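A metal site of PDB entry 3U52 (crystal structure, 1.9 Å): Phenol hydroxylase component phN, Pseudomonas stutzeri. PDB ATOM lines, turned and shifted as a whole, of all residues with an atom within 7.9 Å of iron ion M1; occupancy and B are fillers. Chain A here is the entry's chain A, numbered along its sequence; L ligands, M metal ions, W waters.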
ATOM      1  N   ILE A 104      14.016  25.189  31.938  1.00  0.00           N
ATOM      2  CA  ILE A 104      15.272  24.893  31.215  1.00  0.00           C
ATOM      3  C   ILE A 104      16.254  24.095  32.078  1.00  0.00           C
ATOM      4  O   ILE A 104      16.734  23.027  31.611  1.00  0.00           O
ATOM      5  CB  ILE A 104      15.973  26.131  30.566  1.00  0.00           C
ATOM      6  CG1 ILE A 104      15.175  26.667  29.386  1.00  0.00           C
ATOM      7  CG2 ILE A 104      17.326  25.737  29.976  1.00  0.00           C
ATOM      8  CD1 ILE A 104      14.273  27.825  29.756  1.00  0.00           C
ATOM      9  N   LEU A 107      15.700  20.420  32.138  1.00  0.00           N
ATOM     10  CA  LEU A 107      16.161  19.791  30.903  1.00  0.00           C
ATOM     11  C   LEU A 107      17.642  19.433  30.961  1.00  0.00           C
ATOM     12  O   LEU A 107      18.050  18.412  30.373  1.00  0.00           O
ATOM     13  CB  LEU A 107      15.852  20.699  29.705  1.00  0.00           C
ATOM     14  CG  LEU A 107      14.527  20.423  28.964  1.00  0.00           C
ATOM     15  CD1 LEU A 107      13.486  19.713  29.782  1.00  0.00           C
ATOM     16  CD2 LEU A 107      13.989  21.656  28.218  1.00  0.00           C
ATOM     17  N   GLU A 108      18.444  20.240  31.691  1.00  0.00           N
ATOM     18  CA  GLU A 108      19.891  19.998  31.742  1.00  0.00           C
ATOM     19  C   GLU A 108      19.994  18.631  32.437  1.00  0.00           C
ATOM     20  O   GLU A 108      20.776  17.770  32.046  1.00  0.00           O
ATOM     21  CB  GLU A 108      20.619  21.043  32.604  1.00  0.00           C
ATOM     22  CG  GLU A 108      20.562  22.530  32.116  1.00  0.00           C
ATOM     23  CD  GLU A 108      21.522  22.782  30.979  1.00  0.00           C
ATOM     24  OE1 GLU A 108      21.790  23.950  30.652  1.00  0.00           O
ATOM     25  OE2 GLU A 108      21.996  21.806  30.408  1.00  0.00           O
ATOM     26  N   HIS A 109      19.220  18.477  33.499  1.00  0.00           N
ATOM     27  CA  HIS A 109      19.262  17.272  34.322  1.00  0.00           C
ATOM     28  C   HIS A 109      18.738  16.031  33.569  1.00  0.00           C
ATOM     29  O   HIS A 109      19.362  14.973  33.610  1.00  0.00           O
ATOM     30  CB  HIS A 109      18.487  17.439  35.594  1.00  0.00           C
ATOM     31  CG  HIS A 109      18.926  16.498  36.660  1.00  0.00           C
ATOM     32  ND1 HIS A 109      19.974  16.787  37.514  1.00  0.00           N
ATOM     33  CD2 HIS A 109      18.542  15.247  36.961  1.00  0.00           C
ATOM     34  CE1 HIS A 109      20.171  15.771  38.329  1.00  0.00           C
ATOM     35  NE2 HIS A 109      19.324  14.807  38.001  1.00  0.00           N
ATOM     36  N   ALA A 111      19.058  15.765  30.426  1.00  0.00           N
ATOM     37  CA  ALA A 111      20.064  15.467  29.399  1.00  0.00           C
ATOM     38  C   ALA A 111      21.188  14.650  30.049  1.00  0.00           C
ATOM     39  O   ALA A 111      21.754  13.715  29.434  1.00  0.00           O
ATOM     40  CB  ALA A 111      20.566  16.710  28.785  1.00  0.00           C
ATOM     41  N   PHE A 112      21.471  14.952  31.308  1.00  0.00           N
ATOM     42  CA  PHE A 112      22.457  14.159  32.072  1.00  0.00           C
ATOM     43  C   PHE A 112      22.095  12.655  32.094  1.00  0.00           C
ATOM     44  O   PHE A 112      22.919  11.821  31.774  1.00  0.00           O
ATOM     45  CB  PHE A 112      22.654  14.724  33.480  1.00  0.00           C
ATOM     46  CG  PHE A 112      23.020  13.685  34.500  1.00  0.00           C
ATOM     47  CD1 PHE A 112      24.222  12.923  34.371  1.00  0.00           C
ATOM     48  CD2 PHE A 112      22.212  13.487  35.601  1.00  0.00           C
ATOM     49  CE1 PHE A 112      24.560  11.990  35.303  1.00  0.00           C
ATOM     50  CE2 PHE A 112      22.535  12.502  36.579  1.00  0.00           C
ATOM     51  CZ  PHE A 112      23.715  11.763  36.426  1.00  0.00           C
ATOM     52  N   TYR A 115      21.982  11.223  28.238  1.00  0.00           N
ATOM     53  CA  TYR A 115      23.321  10.978  27.722  1.00  0.00           C
ATOM     54  C   TYR A 115      24.053   9.857  28.483  1.00  0.00           C
ATOM     55  O   TYR A 115      24.830   9.107  27.872  1.00  0.00           O
ATOM     56  CB  TYR A 115      24.164  12.257  27.729  1.00  0.00           C
ATOM     57  CG  TYR A 115      23.928  13.110  26.494  1.00  0.00           C
ATOM     58  CD1 TYR A 115      23.079  14.228  26.565  1.00  0.00           C
ATOM     59  CD2 TYR A 115      24.480  12.752  25.256  1.00  0.00           C
ATOM     60  CE1 TYR A 115      22.820  14.986  25.443  1.00  0.00           C
ATOM     61  CE2 TYR A 115      24.221  13.533  24.107  1.00  0.00           C
ATOM     62  CZ  TYR A 115      23.386  14.633  24.213  1.00  0.00           C
ATOM     63  OH  TYR A 115      23.149  15.413  23.124  1.00  0.00           O
ATOM     64  N   GLN A 134      29.722  14.358  27.615  1.00  0.00           N
ATOM     65  CA  GLN A 134      28.551  15.235  27.529  1.00  0.00           C
ATOM     66  C   GLN A 134      27.610  15.047  28.743  1.00  0.00           C
ATOM     67  O   GLN A 134      27.206  16.008  29.385  1.00  0.00           O
ATOM     68  CB  GLN A 134      27.817  15.065  26.191  1.00  0.00           C
ATOM     69  CG  GLN A 134      26.545  15.838  26.178  1.00  0.00           C
ATOM     70  CD  GLN A 134      26.385  16.737  25.003  1.00  0.00           C
ATOM     71  OE1 GLN A 134      27.097  16.614  23.995  1.00  0.00           O
ATOM     72  NE2 GLN A 134      25.454  17.691  25.121  1.00  0.00           N
ATOM     73  N   ASP A 137      29.059  16.844  31.761  1.00  0.00           N
ATOM     74  CA  ASP A 137      28.863  18.295  31.562  1.00  0.00           C
ATOM     75  C   ASP A 137      27.441  18.760  31.834  1.00  0.00           C
ATOM     76  O   ASP A 137      27.222  19.863  32.365  1.00  0.00           O
ATOM     77  CB  ASP A 137      29.227  18.741  30.124  1.00  0.00           C
ATOM     78  CG  ASP A 137      30.681  18.531  29.752  1.00  0.00           C
ATOM     79  OD1 ASP A 137      31.614  18.376  30.582  1.00  0.00           O
ATOM     80  OD2 ASP A 137      30.890  18.489  28.514  1.00  0.00           O
ATOM     81  N   GLU A 138      26.433  17.991  31.409  1.00  0.00           N
ATOM     82  CA  GLU A 138      25.025  18.378  31.677  1.00  0.00           C
ATOM     83  C   GLU A 138      24.709  18.307  33.168  1.00  0.00           C
ATOM     84  O   GLU A 138      23.944  19.132  33.675  1.00  0.00           O
ATOM     85  CB  GLU A 138      24.044  17.495  30.920  1.00  0.00           C
ATOM     86  CG  GLU A 138      24.385  17.440  29.435  1.00  0.00           C
ATOM     87  CD  GLU A 138      24.110  18.777  28.734  1.00  0.00           C
ATOM     88  OE1 GLU A 138      24.326  18.856  27.524  1.00  0.00           O
ATOM     89  OE2 GLU A 138      23.680  19.759  29.387  1.00  0.00           O
ATOM     90  N   LEU A 139      25.264  17.321  33.871  1.00  0.00           N
ATOM     91  CA  LEU A 139      25.175  17.308  35.311  1.00  0.00           C
ATOM     92  C   LEU A 139      25.754  18.612  35.877  1.00  0.00           C
ATOM     93  O   LEU A 139      25.210  19.231  36.780  1.00  0.00           O
ATOM     94  CB  LEU A 139      25.991  16.134  35.862  1.00  0.00           C
ATOM     95  CG  LEU A 139      25.831  15.995  37.395  1.00  0.00           C
ATOM     96  CD1 LEU A 139      24.323  15.921  37.873  1.00  0.00           C
ATOM     97  CD2 LEU A 139      26.682  14.774  37.935  1.00  0.00           C
ATOM     98  N   ARG A 140      26.903  18.989  35.385  1.00  0.00           N
ATOM     99  CA  ARG A 140      27.495  20.234  35.849  1.00  0.00           C
ATOM    100  C   ARG A 140      26.549  21.396  35.620  1.00  0.00           C
ATOM    101  O   ARG A 140      26.377  22.228  36.491  1.00  0.00           O
ATOM    102  CB  ARG A 140      28.790  20.513  35.100  1.00  0.00           C
ATOM    103  CG  ARG A 140      29.380  21.870  35.525  1.00  0.00           C
ATOM    104  CD  ARG A 140      30.696  22.099  34.955  1.00  0.00           C
ATOM    105  NE  ARG A 140      30.583  23.054  33.923  1.00  0.00           N
ATOM    106  CZ  ARG A 140      31.101  24.264  33.991  1.00  0.00           C
ATOM    107  NH1 ARG A 140      31.792  24.654  35.049  1.00  0.00           N
ATOM    108  NH2 ARG A 140      30.922  25.076  32.964  1.00  0.00           N
ATOM    109  N   HIS A 141      25.942  21.437  34.436  1.00  0.00           N
ATOM    110  CA  HIS A 141      25.094  22.572  34.042  1.00  0.00           C
ATOM    111  C   HIS A 141      23.892  22.649  34.935  1.00  0.00           C
ATOM    112  O   HIS A 141      23.526  23.711  35.409  1.00  0.00           O
ATOM    113  CB  HIS A 141      24.690  22.447  32.549  1.00  0.00           C
ATOM    114  CG  HIS A 141      25.832  22.695  31.609  1.00  0.00           C
ATOM    115  ND1 HIS A 141      25.736  22.514  30.248  1.00  0.00           N
ATOM    116  CD2 HIS A 141      27.115  23.101  31.835  1.00  0.00           C
ATOM    117  CE1 HIS A 141      26.888  22.791  29.673  1.00  0.00           C
ATOM    118  NE2 HIS A 141      27.735  23.171  30.615  1.00  0.00           N
ATOM    119  N   SER A 142      23.324  21.477  35.214  1.00  0.00           N
ATOM    120  CA  SER A 142      22.198  21.347  36.153  1.00  0.00           C
ATOM    121  C   SER A 142      22.524  21.912  37.577  1.00  0.00           C
ATOM    122  O   SER A 142      21.788  22.723  38.128  1.00  0.00           O
ATOM    123  CB  SER A 142      21.879  19.840  36.250  1.00  0.00           C
ATOM    124  OG  SER A 142      20.863  19.643  37.192  1.00  0.00           O
ATOM    125  N   GLN A 145      23.614  25.742  37.745  1.00  0.00           N
ATOM    126  CA  GLN A 145      22.396  26.529  37.664  1.00  0.00           C
ATOM    127  C   GLN A 145      21.621  26.581  38.992  1.00  0.00           C
ATOM    128  O   GLN A 145      21.224  27.658  39.376  1.00  0.00           O
ATOM    129  CB  GLN A 145      21.508  26.037  36.487  1.00  0.00           C
ATOM    130  CG  GLN A 145      22.195  26.381  35.155  1.00  0.00           C
ATOM    131  CD  GLN A 145      21.565  25.688  33.965  1.00  0.00           C
ATOM    132  OE1 GLN A 145      20.467  25.161  34.102  1.00  0.00           O
ATOM    133  NE2 GLN A 145      22.244  25.709  32.795  1.00  0.00           N
ATOM    134  N   PHE A 198      19.178  20.217  18.749  1.00  0.00           N
ATOM    135  CA  PHE A 198      19.160  21.098  19.911  1.00  0.00           C
ATOM    136  C   PHE A 198      20.550  21.725  20.021  1.00  0.00           C
ATOM    137  O   PHE A 198      20.701  22.958  19.895  1.00  0.00           O
ATOM    138  CB  PHE A 198      18.880  20.203  21.138  1.00  0.00           C
ATOM    139  CG  PHE A 198      18.147  20.845  22.300  1.00  0.00           C
ATOM    140  CD1 PHE A 198      17.305  21.928  22.165  1.00  0.00           C
ATOM    141  CD2 PHE A 198      18.227  20.244  23.570  1.00  0.00           C
ATOM    142  CE1 PHE A 198      16.641  22.444  23.326  1.00  0.00           C
ATOM    143  CE2 PHE A 198      17.521  20.747  24.690  1.00  0.00           C
ATOM    144  CZ  PHE A 198      16.758  21.835  24.571  1.00  0.00           C
ATOM    145  N   GLU A 199      21.580  20.885  20.204  1.00  0.00           N
ATOM    146  CA  GLU A 199      22.941  21.359  20.573  1.00  0.00           C
ATOM    147  C   GLU A 199      23.752  21.925  19.460  1.00  0.00           C
ATOM    148  O   GLU A 199      24.767  22.536  19.728  1.00  0.00           O
ATOM    149  CB  GLU A 199      23.794  20.248  21.168  1.00  0.00           C
ATOM    150  CG  GLU A 199      23.289  19.728  22.497  1.00  0.00           C
ATOM    151  CD  GLU A 199      23.655  20.669  23.633  1.00  0.00           C
ATOM    152  OE1 GLU A 199      24.391  20.263  24.548  1.00  0.00           O
ATOM    153  OE2 GLU A 199      23.202  21.830  23.603  1.00  0.00           O
ATOM    154  N   PHE A 207      20.775  29.800  24.089  1.00  0.00           N
ATOM    155  CA  PHE A 207      21.928  30.308  24.844  1.00  0.00           C
ATOM    156  C   PHE A 207      22.129  31.804  24.744  1.00  0.00           C
ATOM    157  O   PHE A 207      22.266  32.482  25.768  1.00  0.00           O
ATOM    158  CB  PHE A 207      23.201  29.591  24.330  1.00  0.00           C
ATOM    159  CG  PHE A 207      24.430  29.776  25.204  1.00  0.00           C
ATOM    160  CD1 PHE A 207      25.298  30.848  24.988  1.00  0.00           C
ATOM    161  CD2 PHE A 207      24.733  28.851  26.208  1.00  0.00           C
ATOM    162  CE1 PHE A 207      26.427  31.008  25.796  1.00  0.00           C
ATOM    163  CE2 PHE A 207      25.853  29.001  27.014  1.00  0.00           C
ATOM    164  CZ  PHE A 207      26.705  30.074  26.813  1.00  0.00           C
ATOM    165  N   PHE A 225      27.917  32.112  34.744  1.00  0.00           N
ATOM    166  CA  PHE A 225      27.574  30.765  34.337  1.00  0.00           C
ATOM    167  C   PHE A 225      27.715  30.627  32.804  1.00  0.00           C
ATOM    168  O   PHE A 225      28.352  29.689  32.336  1.00  0.00           O
ATOM    169  CB  PHE A 225      26.164  30.322  34.769  1.00  0.00           C
ATOM    170  CG  PHE A 225      25.752  29.074  34.040  1.00  0.00           C
ATOM    171  CD1 PHE A 225      26.345  27.837  34.385  1.00  0.00           C
ATOM    172  CD2 PHE A 225      24.900  29.131  32.945  1.00  0.00           C
ATOM    173  CE1 PHE A 225      26.044  26.680  33.659  1.00  0.00           C
ATOM    174  CE2 PHE A 225      24.590  27.964  32.218  1.00  0.00           C
ATOM    175  CZ  PHE A 225      25.171  26.745  32.574  1.00  0.00           C
ATOM    176  N   ALA A 229      30.191  28.072  30.597  1.00  0.00           N
ATOM    177  CA  ALA A 229      29.648  27.006  29.797  1.00  0.00           C
ATOM    178  C   ALA A 229      30.086  27.051  28.337  1.00  0.00           C
ATOM    179  O   ALA A 229      29.897  26.066  27.644  1.00  0.00           O
ATOM    180  CB  ALA A 229      28.148  27.022  29.892  1.00  0.00           C
ATOM    181  N   ASP A 232      32.369  24.221  27.165  1.00  0.00           N
ATOM    182  CA  ASP A 232      31.603  22.989  27.201  1.00  0.00           C
ATOM    183  C   ASP A 232      30.810  22.902  25.897  1.00  0.00           C
ATOM    184  O   ASP A 232      30.865  21.888  25.237  1.00  0.00           O
ATOM    185  CB  ASP A 232      30.595  22.944  28.364  1.00  0.00           C
ATOM    186  CG  ASP A 232      31.258  22.893  29.753  1.00  0.00           C
ATOM    187  OD1 ASP A 232      32.444  22.557  29.899  1.00  0.00           O
ATOM    188  OD2 ASP A 232      30.521  23.165  30.729  1.00  0.00           O
ATOM    189  N   GLU A 233      30.103  23.965  25.537  1.00  0.00           N
ATOM    190  CA  GLU A 233      29.207  23.942  24.372  1.00  0.00           C
ATOM    191  C   GLU A 233      29.919  23.814  23.077  1.00  0.00           C
ATOM    192  O   GLU A 233      29.350  23.268  22.139  1.00  0.00           O
ATOM    193  CB  GLU A 233      28.257  25.166  24.287  1.00  0.00           C
ATOM    194  CG  GLU A 233      27.274  25.249  25.452  1.00  0.00           C
ATOM    195  CD  GLU A 233      26.561  23.928  25.784  1.00  0.00           C
ATOM    196  OE1 GLU A 233      26.553  23.570  26.969  1.00  0.00           O
ATOM    197  OE2 GLU A 233      26.017  23.216  24.912  1.00  0.00           O
ATOM    198  N   HIS A 236      30.053  20.258  22.682  1.00  0.00           N
ATOM    199  CA  HIS A 236      28.717  19.692  22.448  1.00  0.00           C
ATOM    200  C   HIS A 236      28.274  19.940  21.003  1.00  0.00           C
ATOM    201  O   HIS A 236      27.677  19.059  20.379  1.00  0.00           O
ATOM    202  CB  HIS A 236      27.703  20.234  23.470  1.00  0.00           C
ATOM    203  CG  HIS A 236      28.070  19.907  24.877  1.00  0.00           C
ATOM    204  ND1 HIS A 236      27.369  20.383  25.966  1.00  0.00           N
ATOM    205  CD2 HIS A 236      29.096  19.182  25.388  1.00  0.00           C
ATOM    206  CE1 HIS A 236      27.922  19.929  27.083  1.00  0.00           C
ATOM    207  NE2 HIS A 236      28.997  19.227  26.762  1.00  0.00           N
HETATM  208  C1  LIG L   1      20.500  19.648  26.324  1.00  0.00           C
HETATM  209  O1  LIG L   1      21.702  19.014  25.954  1.00  0.00           O
HETATM  210  C2  LIG L   1      20.622  20.408  27.639  1.00  0.00           C
HETATM  211  O2  LIG L   1      21.784  21.257  27.722  1.00  0.00           O
HETATM  212  C3  LIG L   1      19.263  21.090  27.866  1.00  0.00           C
HETATM  213  O3  LIG L   1      19.267  22.516  27.794  1.00  0.00           O
HETATM  214 FE    FE M   1      23.806  21.889  29.005  1.00  0.00          FE
HETATM  215 FE    FE M   2      25.344  21.585  25.936  1.00  0.00          FE
HETATM  216  O   HOH W   1      23.177  24.570  28.988  1.00  0.00           O
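Iron ion M1 is bound by OE2 of Glu 138, at 2.2 Å.
OE2 of Glu 108 is bound to iron ion M1, 2.3 Å away.
ND1 of His 141 binds iron ion M1 (2.4 Å).
Iron ion M1 is bound by O2 of the ligand, 2.5 Å away.
Iron ion M1 has four donor atoms within binding distance.
Slightly farther from iron ion M1 lies water W1 (2.8 Å).
The side-chain carboxylate (OD2) of Asp 232 sits at hydrogen-bond distance from a ring nitrogen (NE2) of His 141 (2.8 Å).
The side-chain carboxylate (OE1) of Glu 108 is in hydrogen-bond range of the side-chain amide nitrogen (NE2) of Gln 145, 2.8 Å away.
NE2 of Gln 134 is in hydrogen-bond range of OE1 of Glu 138, 2.9 Å away.
Merely in contact with iron ion M1: Glu 233 (3.8 Å).
Of the 23 residues printed, 4 come within 4 Å of iron ion M1.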
